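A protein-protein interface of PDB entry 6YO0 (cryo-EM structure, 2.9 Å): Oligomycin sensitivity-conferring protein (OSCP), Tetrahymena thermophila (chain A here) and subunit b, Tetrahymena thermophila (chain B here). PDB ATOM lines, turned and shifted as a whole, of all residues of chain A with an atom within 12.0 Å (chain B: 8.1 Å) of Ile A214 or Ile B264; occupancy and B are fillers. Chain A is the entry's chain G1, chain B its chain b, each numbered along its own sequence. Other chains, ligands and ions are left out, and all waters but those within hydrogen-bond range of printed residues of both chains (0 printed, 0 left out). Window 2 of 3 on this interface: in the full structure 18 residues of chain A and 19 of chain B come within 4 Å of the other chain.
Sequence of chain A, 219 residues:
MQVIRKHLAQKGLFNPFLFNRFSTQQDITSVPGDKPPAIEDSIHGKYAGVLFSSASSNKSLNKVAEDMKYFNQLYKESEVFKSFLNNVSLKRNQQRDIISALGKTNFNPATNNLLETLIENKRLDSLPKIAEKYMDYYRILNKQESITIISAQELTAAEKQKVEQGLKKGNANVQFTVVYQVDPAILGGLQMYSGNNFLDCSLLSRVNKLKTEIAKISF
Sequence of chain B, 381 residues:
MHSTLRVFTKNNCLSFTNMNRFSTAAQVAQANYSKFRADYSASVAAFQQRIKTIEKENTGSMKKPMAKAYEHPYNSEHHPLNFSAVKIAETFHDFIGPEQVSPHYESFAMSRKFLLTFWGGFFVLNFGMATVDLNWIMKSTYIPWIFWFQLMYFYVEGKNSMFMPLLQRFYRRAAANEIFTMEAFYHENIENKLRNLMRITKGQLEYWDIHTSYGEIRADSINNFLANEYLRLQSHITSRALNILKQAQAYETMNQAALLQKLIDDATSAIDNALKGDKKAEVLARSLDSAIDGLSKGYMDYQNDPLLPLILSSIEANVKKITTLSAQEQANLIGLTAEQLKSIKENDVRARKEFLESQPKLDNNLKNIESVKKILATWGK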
ATOM      1  N   SER A 205      30.352   3.919   3.839  1.00  0.00           N
ATOM      2  CA  SER A 205      29.868   2.715   3.176  1.00  0.00           C
ATOM      3  C   SER A 205      29.805   1.554   4.153  1.00  0.00           C
ATOM      4  O   SER A 205      28.841   0.780   4.156  1.00  0.00           O
ATOM      5  CB  SER A 205      30.774   2.369   2.001  1.00  0.00           C
ATOM      6  OG  SER A 205      30.370   1.161   1.386  1.00  0.00           O
ATOM      7  N   ARG A 206      30.827   1.423   4.994  1.00  0.00           N
ATOM      8  CA  ARG A 206      30.834   0.370   6.000  1.00  0.00           C
ATOM      9  C   ARG A 206      29.660   0.525   6.956  1.00  0.00           C
ATOM     10  O   ARG A 206      29.009  -0.461   7.319  1.00  0.00           O
ATOM     11  CB  ARG A 206      32.164   0.399   6.752  1.00  0.00           C
ATOM     12  CG  ARG A 206      32.345  -0.679   7.797  1.00  0.00           C
ATOM     13  CD  ARG A 206      32.508  -2.039   7.164  1.00  0.00           C
ATOM     14  NE  ARG A 206      32.932  -3.051   8.120  1.00  0.00           N
ATOM     15  CZ  ARG A 206      33.196  -4.312   7.798  1.00  0.00           C
ATOM     16  NH1 ARG A 206      33.581  -5.166   8.731  1.00  0.00           N
ATOM     17  NH2 ARG A 206      33.070  -4.719   6.544  1.00  0.00           N
ATOM     18  N   VAL A 207      29.366   1.758   7.365  1.00  0.00           N
ATOM     19  CA  VAL A 207      28.242   1.989   8.266  1.00  0.00           C
ATOM     20  C   VAL A 207      26.938   1.536   7.626  1.00  0.00           C
ATOM     21  O   VAL A 207      26.148   0.802   8.231  1.00  0.00           O
ATOM     22  CB  VAL A 207      28.179   3.474   8.657  1.00  0.00           C
ATOM     23  CG1 VAL A 207      26.904   3.762   9.413  1.00  0.00           C
ATOM     24  CG2 VAL A 207      29.387   3.850   9.478  1.00  0.00           C
ATOM     25  N   ASN A 208      26.695   1.961   6.387  1.00  0.00           N
ATOM     26  CA  ASN A 208      25.458   1.591   5.711  1.00  0.00           C
ATOM     27  C   ASN A 208      25.367   0.087   5.500  1.00  0.00           C
ATOM     28  O   ASN A 208      24.312  -0.517   5.724  1.00  0.00           O
ATOM     29  CB  ASN A 208      25.356   2.326   4.380  1.00  0.00           C
ATOM     30  CG  ASN A 208      25.211   3.820   4.554  1.00  0.00           C
ATOM     31  OD1 ASN A 208      24.807   4.295   5.615  1.00  0.00           O
ATOM     32  ND2 ASN A 208      25.539   4.573   3.512  1.00  0.00           N
ATOM     33  N   LYS A 209      26.464  -0.537   5.074  1.00  0.00           N
ATOM     34  CA  LYS A 209      26.448  -1.973   4.822  1.00  0.00           C
ATOM     35  C   LYS A 209      26.083  -2.751   6.080  1.00  0.00           C
ATOM     36  O   LYS A 209      25.262  -3.673   6.032  1.00  0.00           O
ATOM     37  CB  LYS A 209      27.807  -2.418   4.288  1.00  0.00           C
ATOM     38  CG  LYS A 209      27.918  -3.894   3.957  1.00  0.00           C
ATOM     39  CD  LYS A 209      26.996  -4.277   2.814  1.00  0.00           C
ATOM     40  CE  LYS A 209      27.007  -5.775   2.539  1.00  0.00           C
ATOM     41  NZ  LYS A 209      28.361  -6.310   2.229  1.00  0.00           N
ATOM     42  N   LEU A 210      26.675  -2.389   7.217  1.00  0.00           N
ATOM     43  CA  LEU A 210      26.386  -3.100   8.456  1.00  0.00           C
ATOM     44  C   LEU A 210      24.939  -2.911   8.888  1.00  0.00           C
ATOM     45  O   LEU A 210      24.263  -3.877   9.258  1.00  0.00           O
ATOM     46  CB  LEU A 210      27.337  -2.640   9.557  1.00  0.00           C
ATOM     47  CG  LEU A 210      28.682  -3.359   9.651  1.00  0.00           C
ATOM     48  CD1 LEU A 210      29.460  -3.309   8.355  1.00  0.00           C
ATOM     49  CD2 LEU A 210      29.491  -2.751  10.775  1.00  0.00           C
ATOM     50  N   LYS A 211      24.434  -1.678   8.834  1.00  0.00           N
ATOM     51  CA  LYS A 211      23.060  -1.447   9.263  1.00  0.00           C
ATOM     52  C   LYS A 211      22.075  -2.192   8.379  1.00  0.00           C
ATOM     53  O   LYS A 211      21.002  -2.591   8.844  1.00  0.00           O
ATOM     54  CB  LYS A 211      22.737   0.044   9.256  1.00  0.00           C
ATOM     55  CG  LYS A 211      23.552   0.862  10.230  1.00  0.00           C
ATOM     56  CD  LYS A 211      22.938   2.235  10.465  1.00  0.00           C
ATOM     57  CE  LYS A 211      22.714   2.998   9.171  1.00  0.00           C
ATOM     58  NZ  LYS A 211      22.060   4.312   9.402  1.00  0.00           N
ATOM     59  N   THR A 212      22.421  -2.394   7.110  1.00  0.00           N
ATOM     60  CA  THR A 212      21.540  -3.132   6.218  1.00  0.00           C
ATOM     61  C   THR A 212      21.619  -4.630   6.472  1.00  0.00           C
ATOM     62  O   THR A 212      20.588  -5.310   6.506  1.00  0.00           O
ATOM     63  CB  THR A 212      21.896  -2.827   4.767  1.00  0.00           C
ATOM     64  OG1 THR A 212      23.267  -3.160   4.533  1.00  0.00           O
ATOM     65  CG2 THR A 212      21.679  -1.361   4.470  1.00  0.00           C
ATOM     66  N   GLU A 213      22.827  -5.164   6.661  1.00  0.00           N
ATOM     67  CA  GLU A 213      22.956  -6.603   6.855  1.00  0.00           C
ATOM     68  C   GLU A 213      22.392  -7.025   8.202  1.00  0.00           C
ATOM     69  O   GLU A 213      21.797  -8.102   8.324  1.00  0.00           O
ATOM     70  CB  GLU A 213      24.419  -7.015   6.731  1.00  0.00           C
ATOM     71  CG  GLU A 213      25.005  -6.838   5.345  1.00  0.00           C
ATOM     72  CD  GLU A 213      24.235  -7.580   4.269  1.00  0.00           C
ATOM     73  OE1 GLU A 213      23.391  -8.434   4.614  1.00  0.00           O
ATOM     74  OE2 GLU A 213      24.473  -7.310   3.074  1.00  0.00           O
ATOM     75  N   ILE A 214      22.566  -6.189   9.226  1.00  0.00           N
ATOM     76  CA  ILE A 214      22.001  -6.503  10.533  1.00  0.00           C
ATOM     77  C   ILE A 214      20.488  -6.568  10.445  1.00  0.00           C
ATOM     78  O   ILE A 214      19.840  -7.300  11.204  1.00  0.00           O
ATOM     79  CB  ILE A 214      22.464  -5.478  11.581  1.00  0.00           C
ATOM     80  CG1 ILE A 214      23.967  -5.618  11.807  1.00  0.00           C
ATOM     81  CG2 ILE A 214      21.699  -5.674  12.872  1.00  0.00           C
ATOM     82  CD1 ILE A 214      24.541  -4.610  12.769  1.00  0.00           C
ATOM     83  N   ALA A 215      19.896  -5.788   9.545  1.00  0.00           N
ATOM     84  CA  ALA A 215      18.447  -5.798   9.410  1.00  0.00           C
ATOM     85  C   ALA A 215      17.963  -7.107   8.804  1.00  0.00           C
ATOM     86  O   ALA A 215      16.892  -7.604   9.165  1.00  0.00           O
ATOM     87  CB  ALA A 215      17.998  -4.613   8.563  1.00  0.00           C
ATOM     88  N   LYS A 216      18.733  -7.680   7.884  1.00  0.00           N
ATOM     89  CA  LYS A 216      18.312  -8.864   7.151  1.00  0.00           C
ATOM     90  C   LYS A 216      18.675 -10.164   7.856  1.00  0.00           C
ATOM     91  O   LYS A 216      18.583 -11.231   7.239  1.00  0.00           O
ATOM     92  CB  LYS A 216      18.922  -8.862   5.751  1.00  0.00           C
ATOM     93  CG  LYS A 216      18.581  -7.638   4.934  1.00  0.00           C
ATOM     94  CD  LYS A 216      18.971  -7.816   3.475  1.00  0.00           C
ATOM     95  CE  LYS A 216      20.392  -8.320   3.326  1.00  0.00           C
ATOM     96  NZ  LYS A 216      20.993  -7.919   2.030  1.00  0.00           N
ATOM     97  N   ILE A 217      19.096 -10.101   9.120  1.00  0.00           N
ATOM     98  CA  ILE A 217      19.553 -11.301   9.817  1.00  0.00           C
ATOM     99  C   ILE A 217      18.517 -12.411   9.722  1.00  0.00           C
ATOM    100  O   ILE A 217      18.859 -13.592   9.591  1.00  0.00           O
ATOM    101  CB  ILE A 217      19.882 -10.967  11.283  1.00  0.00           C
ATOM    102  CG1 ILE A 217      21.126 -10.081  11.365  1.00  0.00           C
ATOM    103  CG2 ILE A 217      20.070 -12.230  12.092  1.00  0.00           C
ATOM    104  CD1 ILE A 217      22.343 -10.658  10.701  1.00  0.00           C
ATOM    105  N   SER A 218      17.239 -12.054   9.788  1.00  0.00           N
ATOM    106  CA  SER A 218      16.157 -13.026   9.657  1.00  0.00           C
ATOM    107  C   SER A 218      16.191 -14.034  10.801  1.00  0.00           C
ATOM    108  O   SER A 218      15.932 -15.223  10.611  1.00  0.00           O
ATOM    109  CB  SER A 218      16.221 -13.742   8.308  1.00  0.00           C
ATOM    110  OG  SER A 218      17.404 -14.513   8.197  1.00  0.00           O
ATOM    111  N   PHE A 219      16.526 -13.559  11.997  1.00  0.00           N
ATOM    112  CA  PHE A 219      16.568 -14.424  13.169  1.00  0.00           C
ATOM    113  C   PHE A 219      15.255 -15.181  13.333  1.00  0.00           C
ATOM    114  O   PHE A 219      14.822 -15.456  14.451  1.00  0.00           O
ATOM    115  CB  PHE A 219      16.874 -13.620  14.432  1.00  0.00           C
ATOM    116  CG  PHE A 219      16.038 -12.386  14.591  1.00  0.00           C
ATOM    117  CD1 PHE A 219      14.726 -12.470  15.018  1.00  0.00           C
ATOM    118  CD2 PHE A 219      16.579 -11.137  14.348  1.00  0.00           C
ATOM    119  CE1 PHE A 219      13.961 -11.332  15.173  1.00  0.00           C
ATOM    120  CE2 PHE A 219      15.820  -9.994  14.504  1.00  0.00           C
ATOM    121  CZ  PHE A 219      14.512 -10.091  14.919  1.00  0.00           C
ATOM    122  N   ALA B 257      11.390 -13.143  19.333  1.00  0.00           N
ATOM    123  CA  ALA B 257      11.771 -12.218  18.273  1.00  0.00           C
ATOM    124  C   ALA B 257      11.967 -10.808  18.810  1.00  0.00           C
ATOM    125  O   ALA B 257      12.905 -10.108  18.414  1.00  0.00           O
ATOM    126  CB  ALA B 257      10.717 -12.225  17.172  1.00  0.00           C
ATOM    127  N   ALA B 258      11.093 -10.377  19.718  1.00  0.00           N
ATOM    128  CA  ALA B 258      11.220  -9.040  20.282  1.00  0.00           C
ATOM    129  C   ALA B 258      12.512  -8.898  21.070  1.00  0.00           C
ATOM    130  O   ALA B 258      13.174  -7.855  21.012  1.00  0.00           O
ATOM    131  CB  ALA B 258      10.016  -8.732  21.170  1.00  0.00           C
ATOM    132  N   LEU B 259      12.887  -9.936  21.817  1.00  0.00           N
ATOM    133  CA  LEU B 259      14.133  -9.886  22.569  1.00  0.00           C
ATOM    134  C   LEU B 259      15.330  -9.732  21.641  1.00  0.00           C
ATOM    135  O   LEU B 259      16.213  -8.901  21.878  1.00  0.00           O
ATOM    136  CB  LEU B 259      14.273 -11.149  23.414  1.00  0.00           C
ATOM    137  CG  LEU B 259      15.545 -11.252  24.249  1.00  0.00           C
ATOM    138  CD1 LEU B 259      15.653 -10.073  25.195  1.00  0.00           C
ATOM    139  CD2 LEU B 259      15.565 -12.563  25.007  1.00  0.00           C
ATOM    140  N   LEU B 260      15.377 -10.528  20.573  1.00  0.00           N
ATOM    141  CA  LEU B 260      16.485 -10.420  19.631  1.00  0.00           C
ATOM    142  C   LEU B 260      16.472  -9.082  18.909  1.00  0.00           C
ATOM    143  O   LEU B 260      17.530  -8.491  18.668  1.00  0.00           O
ATOM    144  CB  LEU B 260      16.430 -11.570  18.629  1.00  0.00           C
ATOM    145  CG  LEU B 260      16.487 -12.969  19.238  1.00  0.00           C
ATOM    146  CD1 LEU B 260      16.575 -14.019  18.153  1.00  0.00           C
ATOM    147  CD2 LEU B 260      17.659 -13.089  20.191  1.00  0.00           C
ATOM    148  N   GLN B 261      15.286  -8.571  18.580  1.00  0.00           N
ATOM    149  CA  GLN B 261      15.210  -7.268  17.930  1.00  0.00           C
ATOM    150  C   GLN B 261      15.780  -6.183  18.832  1.00  0.00           C
ATOM    151  O   GLN B 261      16.437  -5.249  18.358  1.00  0.00           O
ATOM    152  CB  GLN B 261      13.762  -6.961  17.557  1.00  0.00           C
ATOM    153  CG  GLN B 261      13.551  -5.592  16.945  1.00  0.00           C
ATOM    154  CD  GLN B 261      14.306  -5.421  15.646  1.00  0.00           C
ATOM    155  OE1 GLN B 261      14.727  -6.398  15.028  1.00  0.00           O
ATOM    156  NE2 GLN B 261      14.473  -4.177  15.220  1.00  0.00           N
ATOM    157  N   LYS B 262      15.535  -6.290  20.138  1.00  0.00           N
ATOM    158  CA  LYS B 262      16.127  -5.353  21.083  1.00  0.00           C
ATOM    159  C   LYS B 262      17.645  -5.429  21.046  1.00  0.00           C
ATOM    160  O   LYS B 262      18.333  -4.402  21.091  1.00  0.00           O
ATOM    161  CB  LYS B 262      15.612  -5.646  22.490  1.00  0.00           C
ATOM    162  CG  LYS B 262      16.473  -5.072  23.604  1.00  0.00           C
ATOM    163  CD  LYS B 262      15.801  -5.210  24.962  1.00  0.00           C
ATOM    164  CE  LYS B 262      14.578  -4.314  25.087  1.00  0.00           C
ATOM    165  NZ  LYS B 262      13.966  -4.391  26.440  1.00  0.00           N
ATOM    166  N   LEU B 263      18.184  -6.645  20.966  1.00  0.00           N
ATOM    167  CA  LEU B 263      19.627  -6.822  20.866  1.00  0.00           C
ATOM    168  C   LEU B 263      20.186  -6.108  19.641  1.00  0.00           C
ATOM    169  O   LEU B 263      21.198  -5.404  19.724  1.00  0.00           O
ATOM    170  CB  LEU B 263      19.953  -8.313  20.822  1.00  0.00           C
ATOM    171  CG  LEU B 263      21.407  -8.689  20.574  1.00  0.00           C
ATOM    172  CD1 LEU B 263      22.283  -8.119  21.669  1.00  0.00           C
ATOM    173  CD2 LEU B 263      21.537 -10.193  20.512  1.00  0.00           C
ATOM    174  N   ILE B 264      19.533  -6.278  18.491  1.00  0.00           N
ATOM    175  CA  ILE B 264      20.017  -5.659  17.261  1.00  0.00           C
ATOM    176  C   ILE B 264      19.966  -4.142  17.362  1.00  0.00           C
ATOM    177  O   ILE B 264      20.859  -3.443  16.869  1.00  0.00           O
ATOM    178  CB  ILE B 264      19.206  -6.167  16.056  1.00  0.00           C
ATOM    179  CG1 ILE B 264      19.808  -7.461  15.523  1.00  0.00           C
ATOM    180  CG2 ILE B 264      19.159  -5.127  14.960  1.00  0.00           C
ATOM    181  CD1 ILE B 264      19.896  -8.544  16.545  1.00  0.00           C
ATOM    182  N   ASP B 265      18.930  -3.606  18.004  1.00  0.00           N
ATOM    183  CA  ASP B 265      18.838  -2.158  18.135  1.00  0.00           C
ATOM    184  C   ASP B 265      19.960  -1.604  18.999  1.00  0.00           C
ATOM    185  O   ASP B 265      20.453  -0.500  18.738  1.00  0.00           O
ATOM    186  CB  ASP B 265      17.482  -1.770  18.717  1.00  0.00           C
ATOM    187  CG  ASP B 265      17.281  -0.269  18.770  1.00  0.00           C
ATOM    188  OD1 ASP B 265      17.088   0.344  17.698  1.00  0.00           O
ATOM    189  OD2 ASP B 265      17.321   0.298  19.881  1.00  0.00           O
ATOM    190  N   ASP B 266      20.380  -2.346  20.023  1.00  0.00           N
ATOM    191  CA  ASP B 266      21.524  -1.913  20.816  1.00  0.00           C
ATOM    192  C   ASP B 266      22.789  -1.864  19.971  1.00  0.00           C
ATOM    193  O   ASP B 266      23.598  -0.938  20.100  1.00  0.00           O
ATOM    194  CB  ASP B 266      21.715  -2.845  22.010  1.00  0.00           C
ATOM    195  CG  ASP B 266      22.956  -2.513  22.814  1.00  0.00           C
ATOM    196  OD1 ASP B 266      22.891  -1.598  23.662  1.00  0.00           O
ATOM    197  OD2 ASP B 266      23.999  -3.163  22.594  1.00  0.00           O
ATOM    198  N   ALA B 267      22.976  -2.855  19.096  1.00  0.00           N
ATOM    199  CA  ALA B 267      24.133  -2.852  18.207  1.00  0.00           C
ATOM    200  C   ALA B 267      24.120  -1.637  17.288  1.00  0.00           C
ATOM    201  O   ALA B 267      25.143  -0.965  17.116  1.00  0.00           O
ATOM    202  CB  ALA B 267      24.159  -4.143  17.390  1.00  0.00           C
ATOM    203  N   THR B 268      22.965  -1.334  16.695  1.00  0.00           N
ATOM    204  CA  THR B 268      22.873  -0.173  15.818  1.00  0.00           C
ATOM    205  C   THR B 268      23.148   1.111  16.584  1.00  0.00           C
ATOM    206  O   THR B 268      23.821   2.017  16.079  1.00  0.00           O
ATOM    207  CB  THR B 268      21.495  -0.115  15.162  1.00  0.00           C
ATOM    208  OG1 THR B 268      20.489   0.020  16.172  1.00  0.00           O
ATOM    209  CG2 THR B 268      21.235  -1.371  14.353  1.00  0.00           C
ATOM    210  N   SER B 269      22.637   1.206  17.811  1.00  0.00           N
ATOM    211  CA  SER B 269      22.889   2.385  18.628  1.00  0.00           C
ATOM    212  C   SER B 269      24.367   2.515  18.968  1.00  0.00           C
ATOM    213  O   SER B 269      24.889   3.632  19.051  1.00  0.00           O
ATOM    214  CB  SER B 269      22.056   2.323  19.905  1.00  0.00           C
ATOM    215  OG  SER B 269      22.332   1.138  20.629  1.00  0.00           O
ATOM    216  N   ALA B 270      25.056   1.389  19.159  1.00  0.00           N
ATOM    217  CA  ALA B 270      26.492   1.444  19.411  1.00  0.00           C
ATOM    218  C   ALA B 270      27.231   2.037  18.223  1.00  0.00           C
ATOM    219  O   ALA B 270      28.133   2.866  18.394  1.00  0.00           O
ATOM    220  CB  ALA B 270      27.022   0.047  19.722  1.00  0.00           C
ATOM    221  N   ILE B 271      26.867   1.626  17.008  1.00  0.00           N
ATOM    222  CA  ILE B 271      27.460   2.231  15.820  1.00  0.00           C
ATOM    223  C   ILE B 271      27.221   3.732  15.831  1.00  0.00           C
ATOM    224  O   ILE B 271      28.148   4.530  15.656  1.00  0.00           O
ATOM    225  CB  ILE B 271      26.899   1.584  14.543  1.00  0.00           C
ATOM    226  CG1 ILE B 271      27.196   0.088  14.537  1.00  0.00           C
ATOM    227  CG2 ILE B 271      27.500   2.238  13.313  1.00  0.00           C
ATOM    228  CD1 ILE B 271      26.652  -0.626  13.330  1.00  0.00           C
ATOM    229  N   LEU B 308      33.272  -3.385  13.475  1.00  0.00           N
ATOM    230  CA  LEU B 308      32.816  -4.756  13.679  1.00  0.00           C
ATOM    231  C   LEU B 308      33.242  -5.309  15.029  1.00  0.00           C
ATOM    232  O   LEU B 308      32.391  -5.874  15.737  1.00  0.00           O
ATOM    233  CB  LEU B 308      33.326  -5.631  12.532  1.00  0.00           C
ATOM    234  CG  LEU B 308      32.894  -7.094  12.547  1.00  0.00           C
ATOM    235  CD1 LEU B 308      31.381  -7.191  12.536  1.00  0.00           C
ATOM    236  CD2 LEU B 308      33.485  -7.827  11.361  1.00  0.00           C
ATOM    237  N   ILE B 311      31.046  -3.511  17.712  1.00  0.00           N
ATOM    238  CA  ILE B 311      29.683  -4.027  17.781  1.00  0.00           C
ATOM    239  C   ILE B 311      29.671  -5.409  18.415  1.00  0.00           C
ATOM    240  O   ILE B 311      28.801  -5.731  19.233  1.00  0.00           O
ATOM    241  CB  ILE B 311      29.044  -4.054  16.381  1.00  0.00           C
ATOM    242  CG1 ILE B 311      29.088  -2.673  15.732  1.00  0.00           C
ATOM    243  CG2 ILE B 311      27.617  -4.544  16.468  1.00  0.00           C
ATOM    244  CD1 ILE B 311      28.933  -2.727  14.242  1.00  0.00           C
ATOM    245  N   SER B 314      29.789  -5.348  22.344  1.00  0.00           N
ATOM    246  CA  SER B 314      28.501  -5.114  22.986  1.00  0.00           C
ATOM    247  C   SER B 314      27.610  -6.344  22.877  1.00  0.00           C
ATOM    248  O   SER B 314      26.974  -6.752  23.856  1.00  0.00           O
ATOM    249  CB  SER B 314      27.816  -3.902  22.359  1.00  0.00           C
ATOM    250  OG  SER B 314      27.500  -4.149  21.002  1.00  0.00           O
ATOM    251  N   ILE B 315      27.554  -6.949  21.689  1.00  0.00           N
ATOM    252  CA  ILE B 315      26.681  -8.097  21.473  1.00  0.00           C
ATOM    253  C   ILE B 315      27.151  -9.300  22.281  1.00  0.00           C
ATOM    254  O   ILE B 315      26.334 -10.059  22.816  1.00  0.00           O
ATOM    255  CB  ILE B 315      26.601  -8.415  19.970  1.00  0.00           C
ATOM    256  CG1 ILE B 315      25.858  -7.287  19.249  1.00  0.00           C
ATOM    257  CG2 ILE B 315      25.940  -9.769  19.743  1.00  0.00           C
ATOM    258  CD1 ILE B 315      25.653  -7.518  17.770  1.00  0.00           C
ATOM    259  N   ASN B 318      25.989  -8.840  25.829  1.00  0.00           N
ATOM    260  CA  ASN B 318      24.576  -9.176  25.951  1.00  0.00           C
ATOM    261  C   ASN B 318      24.359 -10.679  25.847  1.00  0.00           C
ATOM    262  O   ASN B 318      23.538 -11.248  26.575  1.00  0.00           O
ATOM    263  CB  ASN B 318      23.771  -8.439  24.882  1.00  0.00           C
ATOM    264  CG  ASN B 318      23.396  -7.033  25.304  1.00  0.00           C
ATOM    265  OD1 ASN B 318      24.054  -6.431  26.150  1.00  0.00           O
ATOM    266  ND2 ASN B 318      22.333  -6.504  24.713  1.00  0.00           N
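Of the printed residues of chain B, Arg A206 touches Leu B308.
Of the printed residues of chain B, Leu A210 touches Ile B311.
Ile A214 touches one residue of chain B.
No residue of chain B comes within 4 Å of Ala A215.
Of the printed residues of chain B, Phe A219 touches Ala B257 (3.6 Å), Leu B260 (3.8 Å) and Gln B261 (3.7 Å).
Of the printed residues of chain A, Ala B257 touches Phe A219 (3.6 Å).
Of the printed residues of chain A, Leu B260 touches Phe A219 (3.8 Å).
Printed residues of chain A within 4 Å of Gln B261: Phe A219.
Lys B262 touches none of the printed residues of chain A.
Ile B264 touches one residue of chain A.
No residue of chain A comes within 4 Å of Asp B265.
No residue of chain A comes within 4 Å of Asp B266.
No residue of chain A comes within 4 Å of Ala B267.
No residue of chain A comes within 4 Å of Thr B268.
Of the printed residues of chain A, Leu B308 touches Arg A206.
The nearest residue of chain B that does not touch Ile A214 is Ile B271 (4.5 Å).
The nearest printed residue of chain A that does not touch Ala B257 is Ser A218 (8.6 Å).
The side-chain hydroxyl (OG) of Ser B314 lies within hydrogen-bond range of the backbone carbonyl oxygen (O) of Ile B311 (2.7 Å).
Of the 15 printed residues of chain A, 4 touch a printed residue of chain B.
Hydrophobic or aromatic side chains of chain A that line the printed part of chain B: Leu A210, Ile A214 and Phe A219.
Of the 20 printed residues of chain B, 6 touch a printed residue of chain A.
Hydrophobic or aromatic side chains of chain B within 4 Å of the printed part of chain A: Ala B257, Leu B260, Ile B264, Leu B308 and Ile B311.
Arg A206 touches Leu B308 (NH1 to CD2, 3.7 Å).
Leu A210 touches Ile B311 (CD2 to CD1, 3.5 Å).
CG2 of Ile A214 touches CG2 of Ile B264 (3.3 Å).
Ala B257 touches Phe A219 (O to CE1, 3.6 Å).
Leu B260 touches Phe A219.
Phe A219 touches Gln B261 (CZ to OE1, 3.7 Å).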
